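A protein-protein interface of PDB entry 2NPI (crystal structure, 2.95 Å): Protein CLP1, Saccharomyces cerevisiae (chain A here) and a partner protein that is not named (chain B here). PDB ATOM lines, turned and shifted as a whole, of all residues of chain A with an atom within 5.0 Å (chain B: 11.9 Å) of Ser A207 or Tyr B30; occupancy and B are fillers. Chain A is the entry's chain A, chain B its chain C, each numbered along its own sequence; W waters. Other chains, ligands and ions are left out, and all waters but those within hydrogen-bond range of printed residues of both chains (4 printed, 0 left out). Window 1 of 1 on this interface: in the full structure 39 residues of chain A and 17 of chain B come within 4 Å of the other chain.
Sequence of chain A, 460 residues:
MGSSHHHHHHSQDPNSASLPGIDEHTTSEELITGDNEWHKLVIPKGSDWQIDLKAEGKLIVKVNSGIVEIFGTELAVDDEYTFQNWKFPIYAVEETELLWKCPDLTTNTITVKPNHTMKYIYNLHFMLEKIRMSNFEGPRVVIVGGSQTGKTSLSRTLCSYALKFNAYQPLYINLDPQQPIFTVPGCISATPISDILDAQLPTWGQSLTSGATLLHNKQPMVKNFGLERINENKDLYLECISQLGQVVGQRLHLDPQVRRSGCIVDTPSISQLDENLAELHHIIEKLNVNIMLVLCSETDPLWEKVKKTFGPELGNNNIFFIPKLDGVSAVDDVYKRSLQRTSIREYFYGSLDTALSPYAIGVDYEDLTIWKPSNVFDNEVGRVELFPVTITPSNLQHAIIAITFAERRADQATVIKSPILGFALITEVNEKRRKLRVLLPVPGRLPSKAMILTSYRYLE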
ATOM      1  N   PHE A 182      24.502 -26.917 -26.278  1.00  0.00           N
ATOM      2  CA  PHE A 182      24.106 -25.499 -26.200  1.00  0.00           C
ATOM      3  C   PHE A 182      24.282 -24.850 -24.817  1.00  0.00           C
ATOM      4  O   PHE A 182      24.186 -23.625 -24.691  1.00  0.00           O
ATOM      5  CB  PHE A 182      22.669 -25.276 -26.703  1.00  0.00           C
ATOM      6  CG  PHE A 182      22.465 -25.622 -28.148  1.00  0.00           C
ATOM      7  CD1 PHE A 182      21.464 -26.512 -28.521  1.00  0.00           C
ATOM      8  CD2 PHE A 182      23.265 -25.056 -29.140  1.00  0.00           C
ATOM      9  CE1 PHE A 182      21.260 -26.837 -29.857  1.00  0.00           C
ATOM     10  CE2 PHE A 182      23.072 -25.375 -30.479  1.00  0.00           C
ATOM     11  CZ  PHE A 182      22.067 -26.268 -30.838  1.00  0.00           C
ATOM     12  N   THR A 183      24.536 -25.666 -23.794  1.00  0.00           N
ATOM     13  CA  THR A 183      24.654 -25.187 -22.415  1.00  0.00           C
ATOM     14  C   THR A 183      25.823 -25.859 -21.707  1.00  0.00           C
ATOM     15  O   THR A 183      26.703 -26.440 -22.346  1.00  0.00           O
ATOM     16  CB  THR A 183      23.373 -25.490 -21.589  1.00  0.00           C
ATOM     17  OG1 THR A 183      22.219 -25.508 -22.442  1.00  0.00           O
ATOM     18  CG2 THR A 183      23.184 -24.460 -20.476  1.00  0.00           C
ATOM     19  N   GLY A 205      26.531 -25.988 -30.930  1.00  0.00           N
ATOM     20  CA  GLY A 205      26.625 -24.550 -31.114  1.00  0.00           C
ATOM     21  C   GLY A 205      26.698 -23.901 -29.750  1.00  0.00           C
ATOM     22  O   GLY A 205      27.232 -24.491 -28.808  1.00  0.00           O
ATOM     23  N   GLN A 206      26.157 -22.690 -29.638  1.00  0.00           N
ATOM     24  CA  GLN A 206      26.141 -21.979 -28.361  1.00  0.00           C
ATOM     25  C   GLN A 206      24.978 -20.989 -28.225  1.00  0.00           C
ATOM     26  O   GLN A 206      24.362 -20.592 -29.220  1.00  0.00           O
ATOM     27  CB  GLN A 206      27.498 -21.307 -28.085  1.00  0.00           C
ATOM     28  CG  GLN A 206      28.178 -20.677 -29.300  1.00  0.00           C
ATOM     29  CD  GLN A 206      29.533 -20.063 -28.972  1.00  0.00           C
ATOM     30  OE1 GLN A 206      29.710 -19.417 -27.935  1.00  0.00           O
ATOM     31  NE2 GLN A 206      30.494 -20.256 -29.862  1.00  0.00           N
ATOM     32  N   SER A 207      24.686 -20.617 -26.977  1.00  0.00           N
ATOM     33  CA  SER A 207      23.632 -19.666 -26.624  1.00  0.00           C
ATOM     34  C   SER A 207      23.901 -18.274 -27.195  1.00  0.00           C
ATOM     35  O   SER A 207      25.004 -17.996 -27.664  1.00  0.00           O
ATOM     36  CB  SER A 207      23.498 -19.595 -25.098  1.00  0.00           C
ATOM     37  OG  SER A 207      22.861 -18.397 -24.675  1.00  0.00           O
ATOM     38  N   LEU A 208      22.893 -17.403 -27.142  1.00  0.00           N
ATOM     39  CA  LEU A 208      23.015 -16.034 -27.641  1.00  0.00           C
ATOM     40  C   LEU A 208      24.107 -15.237 -26.936  1.00  0.00           C
ATOM     41  O   LEU A 208      24.434 -15.513 -25.783  1.00  0.00           O
ATOM     42  CB  LEU A 208      21.684 -15.298 -27.511  1.00  0.00           C
ATOM     43  CG  LEU A 208      20.599 -15.557 -28.555  1.00  0.00           C
ATOM     44  CD1 LEU A 208      19.510 -14.521 -28.376  1.00  0.00           C
ATOM     45  CD2 LEU A 208      21.143 -15.510 -29.979  1.00  0.00           C
ATOM     46  N   THR A 209      24.666 -14.256 -27.643  1.00  0.00           N
ATOM     47  CA  THR A 209      25.724 -13.393 -27.107  1.00  0.00           C
ATOM     48  C   THR A 209      25.379 -11.909 -27.261  1.00  0.00           C
ATOM     49  O   THR A 209      24.418 -11.555 -27.949  1.00  0.00           O
ATOM     50  CB  THR A 209      27.091 -13.682 -27.765  1.00  0.00           C
ATOM     51  OG1 THR A 209      27.039 -13.335 -29.153  1.00  0.00           O
ATOM     52  CG2 THR A 209      27.465 -15.155 -27.626  1.00  0.00           C
ATOM     53  N   ASN A 217      23.443 -17.727 -33.255  1.00  0.00           N
ATOM     54  CA  ASN A 217      23.370 -18.528 -32.039  1.00  0.00           C
ATOM     55  C   ASN A 217      21.939 -18.924 -31.690  1.00  0.00           C
ATOM     56  O   ASN A 217      20.984 -18.460 -32.322  1.00  0.00           O
ATOM     57  CB  ASN A 217      24.028 -17.785 -30.873  1.00  0.00           C
ATOM     58  CG  ASN A 217      25.517 -17.563 -31.084  1.00  0.00           C
ATOM     59  OD1 ASN A 217      26.239 -18.456 -31.539  1.00  0.00           O
ATOM     60  ND2 ASN A 217      25.988 -16.366 -30.743  1.00  0.00           N
ATOM     61  N   LYS A 218      21.794 -19.780 -30.684  1.00  0.00           N
ATOM     62  CA  LYS A 218      20.491 -20.327 -30.329  1.00  0.00           C
ATOM     63  C   LYS A 218      19.972 -19.834 -28.977  1.00  0.00           C
ATOM     64  O   LYS A 218      20.753 -19.460 -28.104  1.00  0.00           O
ATOM     65  CB  LYS A 218      20.538 -21.858 -30.369  1.00  0.00           C
ATOM     66  CG  LYS A 218      20.336 -22.456 -31.754  1.00  0.00           C
ATOM     67  CD  LYS A 218      21.616 -22.455 -32.574  1.00  0.00           C
ATOM     68  CE  LYS A 218      21.330 -22.343 -34.065  1.00  0.00           C
ATOM     69  NZ  LYS A 218      20.586 -23.518 -34.585  1.00  0.00           N
ATOM     70  N   GLN A 219      18.646 -19.819 -28.833  1.00  0.00           N
ATOM     71  CA  GLN A 219      17.974 -19.493 -27.575  1.00  0.00           C
ATOM     72  C   GLN A 219      17.480 -20.763 -26.889  1.00  0.00           C
ATOM     73  O   GLN A 219      16.412 -21.276 -27.226  1.00  0.00           O
ATOM     74  CB  GLN A 219      16.790 -18.564 -27.827  1.00  0.00           C
ATOM     75  CG  GLN A 219      17.140 -17.102 -27.867  1.00  0.00           C
ATOM     76  CD  GLN A 219      17.093 -16.441 -26.503  1.00  0.00           C
ATOM     77  OE1 GLN A 219      17.598 -16.976 -25.515  1.00  0.00           O
ATOM     78  NE2 GLN A 219      16.497 -15.255 -26.448  1.00  0.00           N
ATOM     79  N   PRO A 220      18.253 -21.276 -25.921  1.00  0.00           N
ATOM     80  CA  PRO A 220      17.893 -22.520 -25.257  1.00  0.00           C
ATOM     81  C   PRO A 220      16.914 -22.340 -24.096  1.00  0.00           C
ATOM     82  O   PRO A 220      16.766 -21.239 -23.565  1.00  0.00           O
ATOM     83  CB  PRO A 220      19.238 -23.040 -24.734  1.00  0.00           C
ATOM     84  CG  PRO A 220      20.259 -21.955 -25.026  1.00  0.00           C
ATOM     85  CD  PRO A 220      19.511 -20.731 -25.396  1.00  0.00           C
ATOM     86  N   VAL A 222      16.580 -24.048 -20.568  1.00  0.00           N
ATOM     87  CA  VAL A 222      17.317 -24.915 -19.646  1.00  0.00           C
ATOM     88  C   VAL A 222      16.525 -25.149 -18.358  1.00  0.00           C
ATOM     89  O   VAL A 222      15.770 -24.273 -17.931  1.00  0.00           O
ATOM     90  CB  VAL A 222      18.716 -24.312 -19.344  1.00  0.00           C
ATOM     91  CG1 VAL A 222      19.474 -25.123 -18.300  1.00  0.00           C
ATOM     92  CG2 VAL A 222      19.533 -24.211 -20.624  1.00  0.00           C
ATOM     93  N   TYR A 347      30.895 -22.043 -22.304  1.00  0.00           N
ATOM     94  CA  TYR A 347      29.783 -21.207 -21.848  1.00  0.00           C
ATOM     95  C   TYR A 347      30.247 -19.816 -21.414  1.00  0.00           C
ATOM     96  O   TYR A 347      29.571 -18.820 -21.682  1.00  0.00           O
ATOM     97  CB  TYR A 347      29.028 -21.896 -20.706  1.00  0.00           C
ATOM     98  CG  TYR A 347      27.961 -21.046 -20.037  1.00  0.00           C
ATOM     99  CD1 TYR A 347      26.715 -20.857 -20.634  1.00  0.00           C
ATOM    100  CD2 TYR A 347      28.196 -20.442 -18.800  1.00  0.00           C
ATOM    101  CE1 TYR A 347      25.730 -20.083 -20.020  1.00  0.00           C
ATOM    102  CE2 TYR A 347      27.216 -19.665 -18.180  1.00  0.00           C
ATOM    103  CZ  TYR A 347      25.987 -19.493 -18.796  1.00  0.00           C
ATOM    104  OH  TYR A 347      25.017 -18.728 -18.193  1.00  0.00           O
ATOM    105  N   PHE A 405      15.280 -17.369 -11.386  1.00  0.00           N
ATOM    106  CA  PHE A 405      14.591 -16.086 -11.498  1.00  0.00           C
ATOM    107  C   PHE A 405      13.919 -15.695 -10.187  1.00  0.00           C
ATOM    108  O   PHE A 405      13.574 -14.531  -9.989  1.00  0.00           O
ATOM    109  CB  PHE A 405      13.540 -16.133 -12.606  1.00  0.00           C
ATOM    110  CG  PHE A 405      14.044 -15.687 -13.946  1.00  0.00           C
ATOM    111  CD1 PHE A 405      14.690 -16.580 -14.796  1.00  0.00           C
ATOM    112  CD2 PHE A 405      13.856 -14.375 -14.368  1.00  0.00           C
ATOM    113  CE1 PHE A 405      15.148 -16.170 -16.040  1.00  0.00           C
ATOM    114  CE2 PHE A 405      14.310 -13.954 -15.612  1.00  0.00           C
ATOM    115  CZ  PHE A 405      14.954 -14.855 -16.451  1.00  0.00           C
ATOM    116  N   ILE A 420      15.668 -21.086 -15.034  1.00  0.00           N
ATOM    117  CA  ILE A 420      17.083 -20.800 -14.839  1.00  0.00           C
ATOM    118  C   ILE A 420      17.519 -19.623 -15.708  1.00  0.00           C
ATOM    119  O   ILE A 420      17.243 -19.589 -16.905  1.00  0.00           O
ATOM    120  CB  ILE A 420      17.970 -22.057 -15.075  1.00  0.00           C
ATOM    121  CG1 ILE A 420      18.046 -22.916 -13.804  1.00  0.00           C
ATOM    122  CG2 ILE A 420      19.393 -21.662 -15.459  1.00  0.00           C
ATOM    123  CD1 ILE A 420      16.801 -23.729 -13.475  1.00  0.00           C
ATOM    124  N   LEU A 421      18.185 -18.659 -15.077  1.00  0.00           N
ATOM    125  CA  LEU A 421      18.664 -17.443 -15.730  1.00  0.00           C
ATOM    126  C   LEU A 421      19.983 -17.702 -16.460  1.00  0.00           C
ATOM    127  O   LEU A 421      20.166 -17.284 -17.608  1.00  0.00           O
ATOM    128  CB  LEU A 421      18.838 -16.334 -14.686  1.00  0.00           C
ATOM    129  CG  LEU A 421      19.413 -14.971 -15.080  1.00  0.00           C
ATOM    130  CD1 LEU A 421      18.336 -14.045 -15.616  1.00  0.00           C
ATOM    131  CD2 LEU A 421      20.105 -14.330 -13.891  1.00  0.00           C
ATOM    132  N   GLY A 422      20.894 -18.392 -15.782  1.00  0.00           N
ATOM    133  CA  GLY A 422      22.209 -18.704 -16.321  1.00  0.00           C
ATOM    134  C   GLY A 422      23.041 -19.359 -15.243  1.00  0.00           C
ATOM    135  O   GLY A 422      22.532 -19.674 -14.168  1.00  0.00           O
ATOM    136  N   PHE A 423      24.324 -19.557 -15.519  1.00  0.00           N
ATOM    137  CA  PHE A 423      25.199 -20.253 -14.587  1.00  0.00           C
ATOM    138  C   PHE A 423      26.377 -19.381 -14.168  1.00  0.00           C
ATOM    139  O   PHE A 423      26.755 -18.452 -14.883  1.00  0.00           O
ATOM    140  CB  PHE A 423      25.689 -21.574 -15.195  1.00  0.00           C
ATOM    141  CG  PHE A 423      24.587 -22.565 -15.469  1.00  0.00           C
ATOM    142  CD1 PHE A 423      23.870 -22.520 -16.660  1.00  0.00           C
ATOM    143  CD2 PHE A 423      24.270 -23.545 -14.538  1.00  0.00           C
ATOM    144  CE1 PHE A 423      22.849 -23.431 -16.915  1.00  0.00           C
ATOM    145  CE2 PHE A 423      23.252 -24.466 -14.786  1.00  0.00           C
ATOM    146  CZ  PHE A 423      22.541 -24.409 -15.976  1.00  0.00           C
ATOM    147  N   GLN B  25      32.814  -9.222 -26.774  1.00  0.00           N
ATOM    148  CA  GLN B  25      31.437  -9.670 -26.553  1.00  0.00           C
ATOM    149  C   GLN B  25      31.307 -10.457 -25.252  1.00  0.00           C
ATOM    150  O   GLN B  25      32.303 -10.722 -24.578  1.00  0.00           O
ATOM    151  CB  GLN B  25      30.965 -10.548 -27.713  1.00  0.00           C
ATOM    152  CG  GLN B  25      30.653  -9.812 -28.999  1.00  0.00           C
ATOM    153  CD  GLN B  25      29.829 -10.655 -29.950  1.00  0.00           C
ATOM    154  OE1 GLN B  25      28.831 -11.254 -29.556  1.00  0.00           O
ATOM    155  NE2 GLN B  25      30.243 -10.705 -31.211  1.00  0.00           N
ATOM    156  N   SER B  26      30.074 -10.837 -24.915  1.00  0.00           N
ATOM    157  CA  SER B  26      29.792 -11.621 -23.713  1.00  0.00           C
ATOM    158  C   SER B  26      28.566 -12.515 -23.886  1.00  0.00           C
ATOM    159  O   SER B  26      27.712 -12.248 -24.732  1.00  0.00           O
ATOM    160  CB  SER B  26      29.581 -10.697 -22.516  1.00  0.00           C
ATOM    161  OG  SER B  26      30.769  -9.997 -22.196  1.00  0.00           O
ATOM    162  N   ARG B  27      28.490 -13.571 -23.076  1.00  0.00           N
ATOM    163  CA  ARG B  27      27.321 -14.451 -23.026  1.00  0.00           C
ATOM    164  C   ARG B  27      26.110 -13.691 -22.482  1.00  0.00           C
ATOM    165  O   ARG B  27      26.263 -12.714 -21.744  1.00  0.00           O
ATOM    166  CB  ARG B  27      27.625 -15.671 -22.146  1.00  0.00           C
ATOM    167  CG  ARG B  27      26.568 -16.779 -22.145  1.00  0.00           C
ATOM    168  CD  ARG B  27      26.503 -17.531 -23.474  1.00  0.00           C
ATOM    169  NE  ARG B  27      27.664 -18.396 -23.692  1.00  0.00           N
ATOM    170  CZ  ARG B  27      28.043 -18.861 -24.882  1.00  0.00           C
ATOM    171  NH1 ARG B  27      27.368 -18.544 -25.979  1.00  0.00           N
ATOM    172  NH2 ARG B  27      29.110 -19.638 -24.978  1.00  0.00           N
ATOM    173  N   ASN B  28      24.914 -14.133 -22.868  1.00  0.00           N
ATOM    174  CA  ASN B  28      23.665 -13.543 -22.386  1.00  0.00           C
ATOM    175  C   ASN B  28      22.961 -14.430 -21.380  1.00  0.00           C
ATOM    176  O   ASN B  28      23.163 -15.648 -21.366  1.00  0.00           O
ATOM    177  CB  ASN B  28      22.709 -13.267 -23.547  1.00  0.00           C
ATOM    178  CG  ASN B  28      23.076 -12.028 -24.326  1.00  0.00           C
ATOM    179  OD1 ASN B  28      24.236 -11.612 -24.352  1.00  0.00           O
ATOM    180  ND2 ASN B  28      22.088 -11.433 -24.977  1.00  0.00           N
ATOM    181  N   TRP B  29      22.128 -13.813 -20.546  1.00  0.00           N
ATOM    182  CA  TRP B  29      21.234 -14.553 -19.670  1.00  0.00           C
ATOM    183  C   TRP B  29      20.139 -15.194 -20.514  1.00  0.00           C
ATOM    184  O   TRP B  29      19.805 -14.693 -21.588  1.00  0.00           O
ATOM    185  CB  TRP B  29      20.608 -13.630 -18.623  1.00  0.00           C
ATOM    186  CG  TRP B  29      21.585 -13.016 -17.653  1.00  0.00           C
ATOM    187  CD1 TRP B  29      21.841 -11.688 -17.488  1.00  0.00           C
ATOM    188  CD2 TRP B  29      22.421 -13.705 -16.708  1.00  0.00           C
ATOM    189  NE1 TRP B  29      22.783 -11.502 -16.505  1.00  0.00           N
ATOM    190  CE2 TRP B  29      23.157 -12.723 -16.009  1.00  0.00           C
ATOM    191  CE3 TRP B  29      22.624 -15.056 -16.388  1.00  0.00           C
ATOM    192  CZ2 TRP B  29      24.081 -13.045 -15.011  1.00  0.00           C
ATOM    193  CZ3 TRP B  29      23.539 -15.376 -15.390  1.00  0.00           C
ATOM    194  CH2 TRP B  29      24.256 -14.373 -14.713  1.00  0.00           C
ATOM    195  N   TYR B  30      19.586 -16.304 -20.033  1.00  0.00           N
ATOM    196  CA  TYR B  30      18.449 -16.928 -20.699  1.00  0.00           C
ATOM    197  C   TYR B  30      17.153 -16.160 -20.416  1.00  0.00           C
ATOM    198  O   TYR B  30      17.086 -15.363 -19.477  1.00  0.00           O
ATOM    199  CB  TYR B  30      18.298 -18.390 -20.270  1.00  0.00           C
ATOM    200  CG  TYR B  30      19.543 -19.233 -20.425  1.00  0.00           C
ATOM    201  CD1 TYR B  30      20.073 -19.926 -19.338  1.00  0.00           C
ATOM    202  CD2 TYR B  30      20.186 -19.347 -21.657  1.00  0.00           C
ATOM    203  CE1 TYR B  30      21.214 -20.708 -19.472  1.00  0.00           C
ATOM    204  CE2 TYR B  30      21.327 -20.127 -21.802  1.00  0.00           C
ATOM    205  CZ  TYR B  30      21.835 -20.802 -20.706  1.00  0.00           C
ATOM    206  OH  TYR B  30      22.964 -21.570 -20.842  1.00  0.00           O
ATOM    207  N   LEU B  31      16.135 -16.401 -21.240  1.00  0.00           N
ATOM    208  CA  LEU B  31      14.822 -15.796 -21.042  1.00  0.00           C
ATOM    209  C   LEU B  31      14.038 -16.570 -19.998  1.00  0.00           C
ATOM    210  O   LEU B  31      14.298 -17.751 -19.770  1.00  0.00           O
ATOM    211  CB  LEU B  31      14.030 -15.769 -22.351  1.00  0.00           C
ATOM    212  CG  LEU B  31      14.611 -15.097 -23.597  1.00  0.00           C
ATOM    213  CD1 LEU B  31      13.575 -15.122 -24.704  1.00  0.00           C
ATOM    214  CD2 LEU B  31      15.070 -13.664 -23.327  1.00  0.00           C
ATOM    215  N   SER B  32      13.075 -15.900 -19.371  1.00  0.00           N
ATOM    216  CA  SER B  32      12.186 -16.545 -18.415  1.00  0.00           C
ATOM    217  C   SER B  32      11.227 -17.482 -19.149  1.00  0.00           C
ATOM    218  O   SER B  32      11.193 -17.495 -20.384  1.00  0.00           O
ATOM    219  CB  SER B  32      11.402 -15.498 -17.633  1.00  0.00           C
ATOM    220  OG  SER B  32      10.318 -15.010 -18.400  1.00  0.00           O
ATOM    221  N   ASP B  33      10.446 -18.248 -18.388  1.00  0.00           N
ATOM    222  CA  ASP B  33       9.534 -19.249 -18.948  1.00  0.00           C
ATOM    223  C   ASP B  33       8.551 -18.668 -19.964  1.00  0.00           C
ATOM    224  O   ASP B  33       8.515 -19.105 -21.119  1.00  0.00           O
ATOM    225  CB  ASP B  33       8.787 -19.998 -17.836  1.00  0.00           C
ATOM    226  CG  ASP B  33       9.605 -21.142 -17.242  1.00  0.00           C
ATOM    227  OD1 ASP B  33      10.532 -21.645 -17.919  1.00  0.00           O
ATOM    228  OD2 ASP B  33       9.310 -21.543 -16.095  1.00  0.00           O
ATOM    229  N   SER B  34       7.772 -17.678 -19.529  1.00  0.00           N
ATOM    230  CA  SER B  34       6.794 -17.008 -20.389  1.00  0.00           C
ATOM    231  C   SER B  34       7.465 -16.256 -21.537  1.00  0.00           C
ATOM    232  O   SER B  34       6.988 -16.283 -22.672  1.00  0.00           O
ATOM    233  CB  SER B  34       5.955 -16.039 -19.563  1.00  0.00           C
ATOM    234  OG  SER B  34       6.782 -15.056 -18.961  1.00  0.00           O
ATOM    235  N   GLN B  35       8.581 -15.600 -21.224  1.00  0.00           N
ATOM    236  CA  GLN B  35       9.324 -14.773 -22.174  1.00  0.00           C
ATOM    237  C   GLN B  35       9.922 -15.571 -23.336  1.00  0.00           C
ATOM    238  O   GLN B  35      10.024 -15.060 -24.455  1.00  0.00           O
ATOM    239  CB  GLN B  35      10.430 -14.027 -21.432  1.00  0.00           C
ATOM    240  CG  GLN B  35      10.889 -12.745 -22.085  1.00  0.00           C
ATOM    241  CD  GLN B  35      11.680 -11.881 -21.122  1.00  0.00           C
ATOM    242  OE1 GLN B  35      11.140 -11.384 -20.131  1.00  0.00           O
ATOM    243  NE2 GLN B  35      12.969 -11.696 -21.407  1.00  0.00           N
ATOM    244  N   TRP B  36      10.324 -16.810 -23.062  1.00  0.00           N
ATOM    245  CA  TRP B  36      10.860 -17.701 -24.088  1.00  0.00           C
ATOM    246  C   TRP B  36       9.744 -18.212 -24.990  1.00  0.00           C
ATOM    247  O   TRP B  36       9.941 -18.395 -26.190  1.00  0.00           O
ATOM    248  CB  TRP B  36      11.593 -18.878 -23.439  1.00  0.00           C
ATOM    249  CG  TRP B  36      12.198 -19.873 -24.412  1.00  0.00           C
ATOM    250  CD1 TRP B  36      13.396 -19.765 -25.058  1.00  0.00           C
ATOM    251  CD2 TRP B  36      11.636 -21.131 -24.821  1.00  0.00           C
ATOM    252  NE1 TRP B  36      13.613 -20.870 -25.848  1.00  0.00           N
ATOM    253  CE2 TRP B  36      12.551 -21.724 -25.720  1.00  0.00           C
ATOM    254  CE3 TRP B  36      10.449 -21.813 -24.515  1.00  0.00           C
ATOM    255  CZ2 TRP B  36      12.317 -22.968 -26.319  1.00  0.00           C
ATOM    256  CZ3 TRP B  36      10.218 -23.051 -25.110  1.00  0.00           C
ATOM    257  CH2 TRP B  36      11.148 -23.612 -26.003  1.00  0.00           C
ATOM    258  N   ALA B  37       8.575 -18.436 -24.397  1.00  0.00           N
ATOM    259  CA  ALA B  37       7.421 -18.959 -25.115  1.00  0.00           C
ATOM    260  C   ALA B  37       6.932 -17.970 -26.165  1.00  0.00           C
ATOM    261  O   ALA B  37       6.475 -18.369 -27.235  1.00  0.00           O
ATOM    262  CB  ALA B  37       6.311 -19.294 -24.139  1.00  0.00           C
ATOM    263  N   ALA B  38       7.038 -16.682 -25.853  1.00  0.00           N
ATOM    264  CA  ALA B  38       6.650 -15.629 -26.782  1.00  0.00           C
ATOM    265  C   ALA B  38       7.720 -15.371 -27.849  1.00  0.00           C
ATOM    266  O   ALA B  38       7.408 -14.864 -28.929  1.00  0.00           O
ATOM    267  CB  ALA B  38       6.323 -14.347 -26.022  1.00  0.00           C
ATOM    268  N   PHE B  39       8.968 -15.737 -27.549  1.00  0.00           N
ATOM    269  CA  PHE B  39      10.115 -15.467 -28.429  1.00  0.00           C
ATOM    270  C   PHE B  39      10.016 -16.134 -29.799  1.00  0.00           C
ATOM    271  O   PHE B  39       9.617 -17.293 -29.912  1.00  0.00           O
ATOM    272  CB  PHE B  39      11.424 -15.879 -27.747  1.00  0.00           C
ATOM    273  CG  PHE B  39      12.659 -15.379 -28.445  1.00  0.00           C
ATOM    274  CD1 PHE B  39      13.083 -14.061 -28.282  1.00  0.00           C
ATOM    275  CD2 PHE B  39      13.405 -16.227 -29.255  1.00  0.00           C
ATOM    276  CE1 PHE B  39      14.229 -13.593 -28.922  1.00  0.00           C
ATOM    277  CE2 PHE B  39      14.551 -15.767 -29.900  1.00  0.00           C
ATOM    278  CZ  PHE B  39      14.964 -14.448 -29.730  1.00  0.00           C
ATOM    279  N   ASP B  41      12.338 -16.972 -33.259  1.00  0.00           N
ATOM    280  CA  ASP B  41      13.741 -17.076 -33.660  1.00  0.00           C
ATOM    281  C   ASP B  41      14.089 -16.214 -34.879  1.00  0.00           C
ATOM    282  O   ASP B  41      15.258 -16.103 -35.256  1.00  0.00           O
ATOM    283  CB  ASP B  41      14.171 -18.540 -33.830  1.00  0.00           C
ATOM    284  CG  ASP B  41      14.505 -19.208 -32.498  1.00  0.00           C
ATOM    285  OD1 ASP B  41      13.571 -19.513 -31.726  1.00  0.00           O
ATOM    286  OD2 ASP B  41      15.702 -19.430 -32.215  1.00  0.00           O
ATOM    287  N   ILE B  44      16.448 -13.435 -33.936  1.00  0.00           N
ATOM    288  CA  ILE B  44      17.861 -13.836 -34.034  1.00  0.00           C
ATOM    289  C   ILE B  44      18.378 -13.699 -35.473  1.00  0.00           C
ATOM    290  O   ILE B  44      19.477 -13.190 -35.698  1.00  0.00           O
ATOM    291  CB  ILE B  44      18.088 -15.298 -33.546  1.00  0.00           C
ATOM    292  CG1 ILE B  44      17.694 -15.456 -32.071  1.00  0.00           C
ATOM    293  CG2 ILE B  44      19.545 -15.743 -33.788  1.00  0.00           C
ATOM    294  CD1 ILE B  44      17.685 -16.902 -31.577  1.00  0.00           C
HETATM  295  O   HOH W   1      22.551 -17.731 -19.941  1.00  0.00           O
HETATM  296  O   HOH W   2      17.210 -21.384 -30.912  1.00  0.00           O
HETATM  297  O   HOH W   3      14.356 -20.176 -28.813  1.00  0.00           O
HETATM  298  O   HOH W   4      24.436 -21.750 -22.875  1.00  0.00           O
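The backbone carbonyl oxygen of Tyr A347 is in hydrogen-bond range of the guanidinium group of Arg B27. The backbone carbonyl oxygen (O) of Ser A207 sits at hydrogen-bond distance from the guanidinium group (NH1) of Arg B27, 3.0 Å away. N of Tyr B30 is in hydrogen-bond range of O of Leu A421 (2.7 Å). OG1 of Thr A209 sits at hydrogen-bond distance from OE1 of Gln B25 (2.8 Å). The backbone carbonyl oxygen of Leu A208 sits at hydrogen-bond distance from the backbone NH of Asn B28 (3.3 Å). O of Gln A219 is in hydrogen-bond range of NE1 of Trp B36 (3.1 Å). The side-chain amide oxygen (OE1) of Gln A206 sits at hydrogen-bond distance from the guanidinium group (NH2) of Arg B27, 3.0 Å away.
The side-chain hydroxyl (OG) of Ser B32 lies close to the backbone NH (N) of Gln B35, 3.4 Å away. The backbone carbonyl oxygen (O) of Gln A206 lies within hydrogen-bond range of the backbone NH (N) of Lys A218, 3.1 Å away. The backbone NH (N) of Leu A208 lies within hydrogen-bond range of the backbone carbonyl oxygen (O) of Lys A218 (3.1 Å). N of Phe A423 is in hydrogen-bond range of OH of Tyr A347 (2.9 Å).
OH of Tyr B30 touches CG2 of Thr A183, at 2.9 Å. Arg B27 touches Leu A208. O of Ser B26 touches CA of Thr A209, at 3.3 Å. Arg B27 touches Thr A209 (NH1 to CG2, 3.8 Å). Asn B28 touches Thr A209. Tyr B30 touches Pro A220. CE1 of Tyr A347 touches OH of Tyr B30, 3.2 Å away. N of Ser B32 touches CZ of Phe A405 (3.6 Å). Ile A420 touches Tyr B30 (O to CB, 3.7 Å). Trp B29 touches Gly A422.
Of the printed residues of chain B, Ser A207 touches Arg B27 and Tyr B30. Of chain B, only Tyr B30 comes within 4 Å of Thr A183. Asn A217 touches just one residue of chain B: Ile B44 (3.4 Å). Of chain B, only Tyr B30 comes within 4 Å of Ile A420. Gly A422 touches just these residues of chain B: Trp B29 and Tyr B30. Printed residues of chain A within 4 Å of Arg B27: Gln A206, Ser A207, Leu A208, Thr A209 and Tyr A347. Of the printed residues of chain A, Phe B39 touches Gln A219 (3.6 Å). Of the printed residues of chain A, Ser B32 touches Phe A405 (3.6 Å). Printed residues of chain A within 4 Å of Leu B31: Gln A219 (3.4 Å). The nearest residue of chain B that does not touch Ser A207 is Asn B28 (4.3 Å).
Hydrophobic or aromatic side chains of chain A within 4 Å of the printed part of chain B: Pro A220, Tyr A347, Phe A405 and Leu A421. Along chain B the printed residues that touch a printed residue of chain A span positions 25 to 44. Among the printed residues, no Asp or Glu carboxylate lies within 4 Å of a Lys or Arg side-chain nitrogen of the other chain.
Water W4 bridges the side-chain hydroxyl of Tyr B30 and the backbone carbonyl oxygen of Phe A182. Water W1 lies within hydrogen-bond range of O of Asn B28, OH of Tyr A347, N of Tyr B30 and O of Leu A421. Water W3 lies within hydrogen-bond range of the backbone carbonyl oxygen (O) of Gln A219, the side-chain carboxylate (OD1) of Asp B41 and the indole nitrogen (NE1) of Trp B36.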
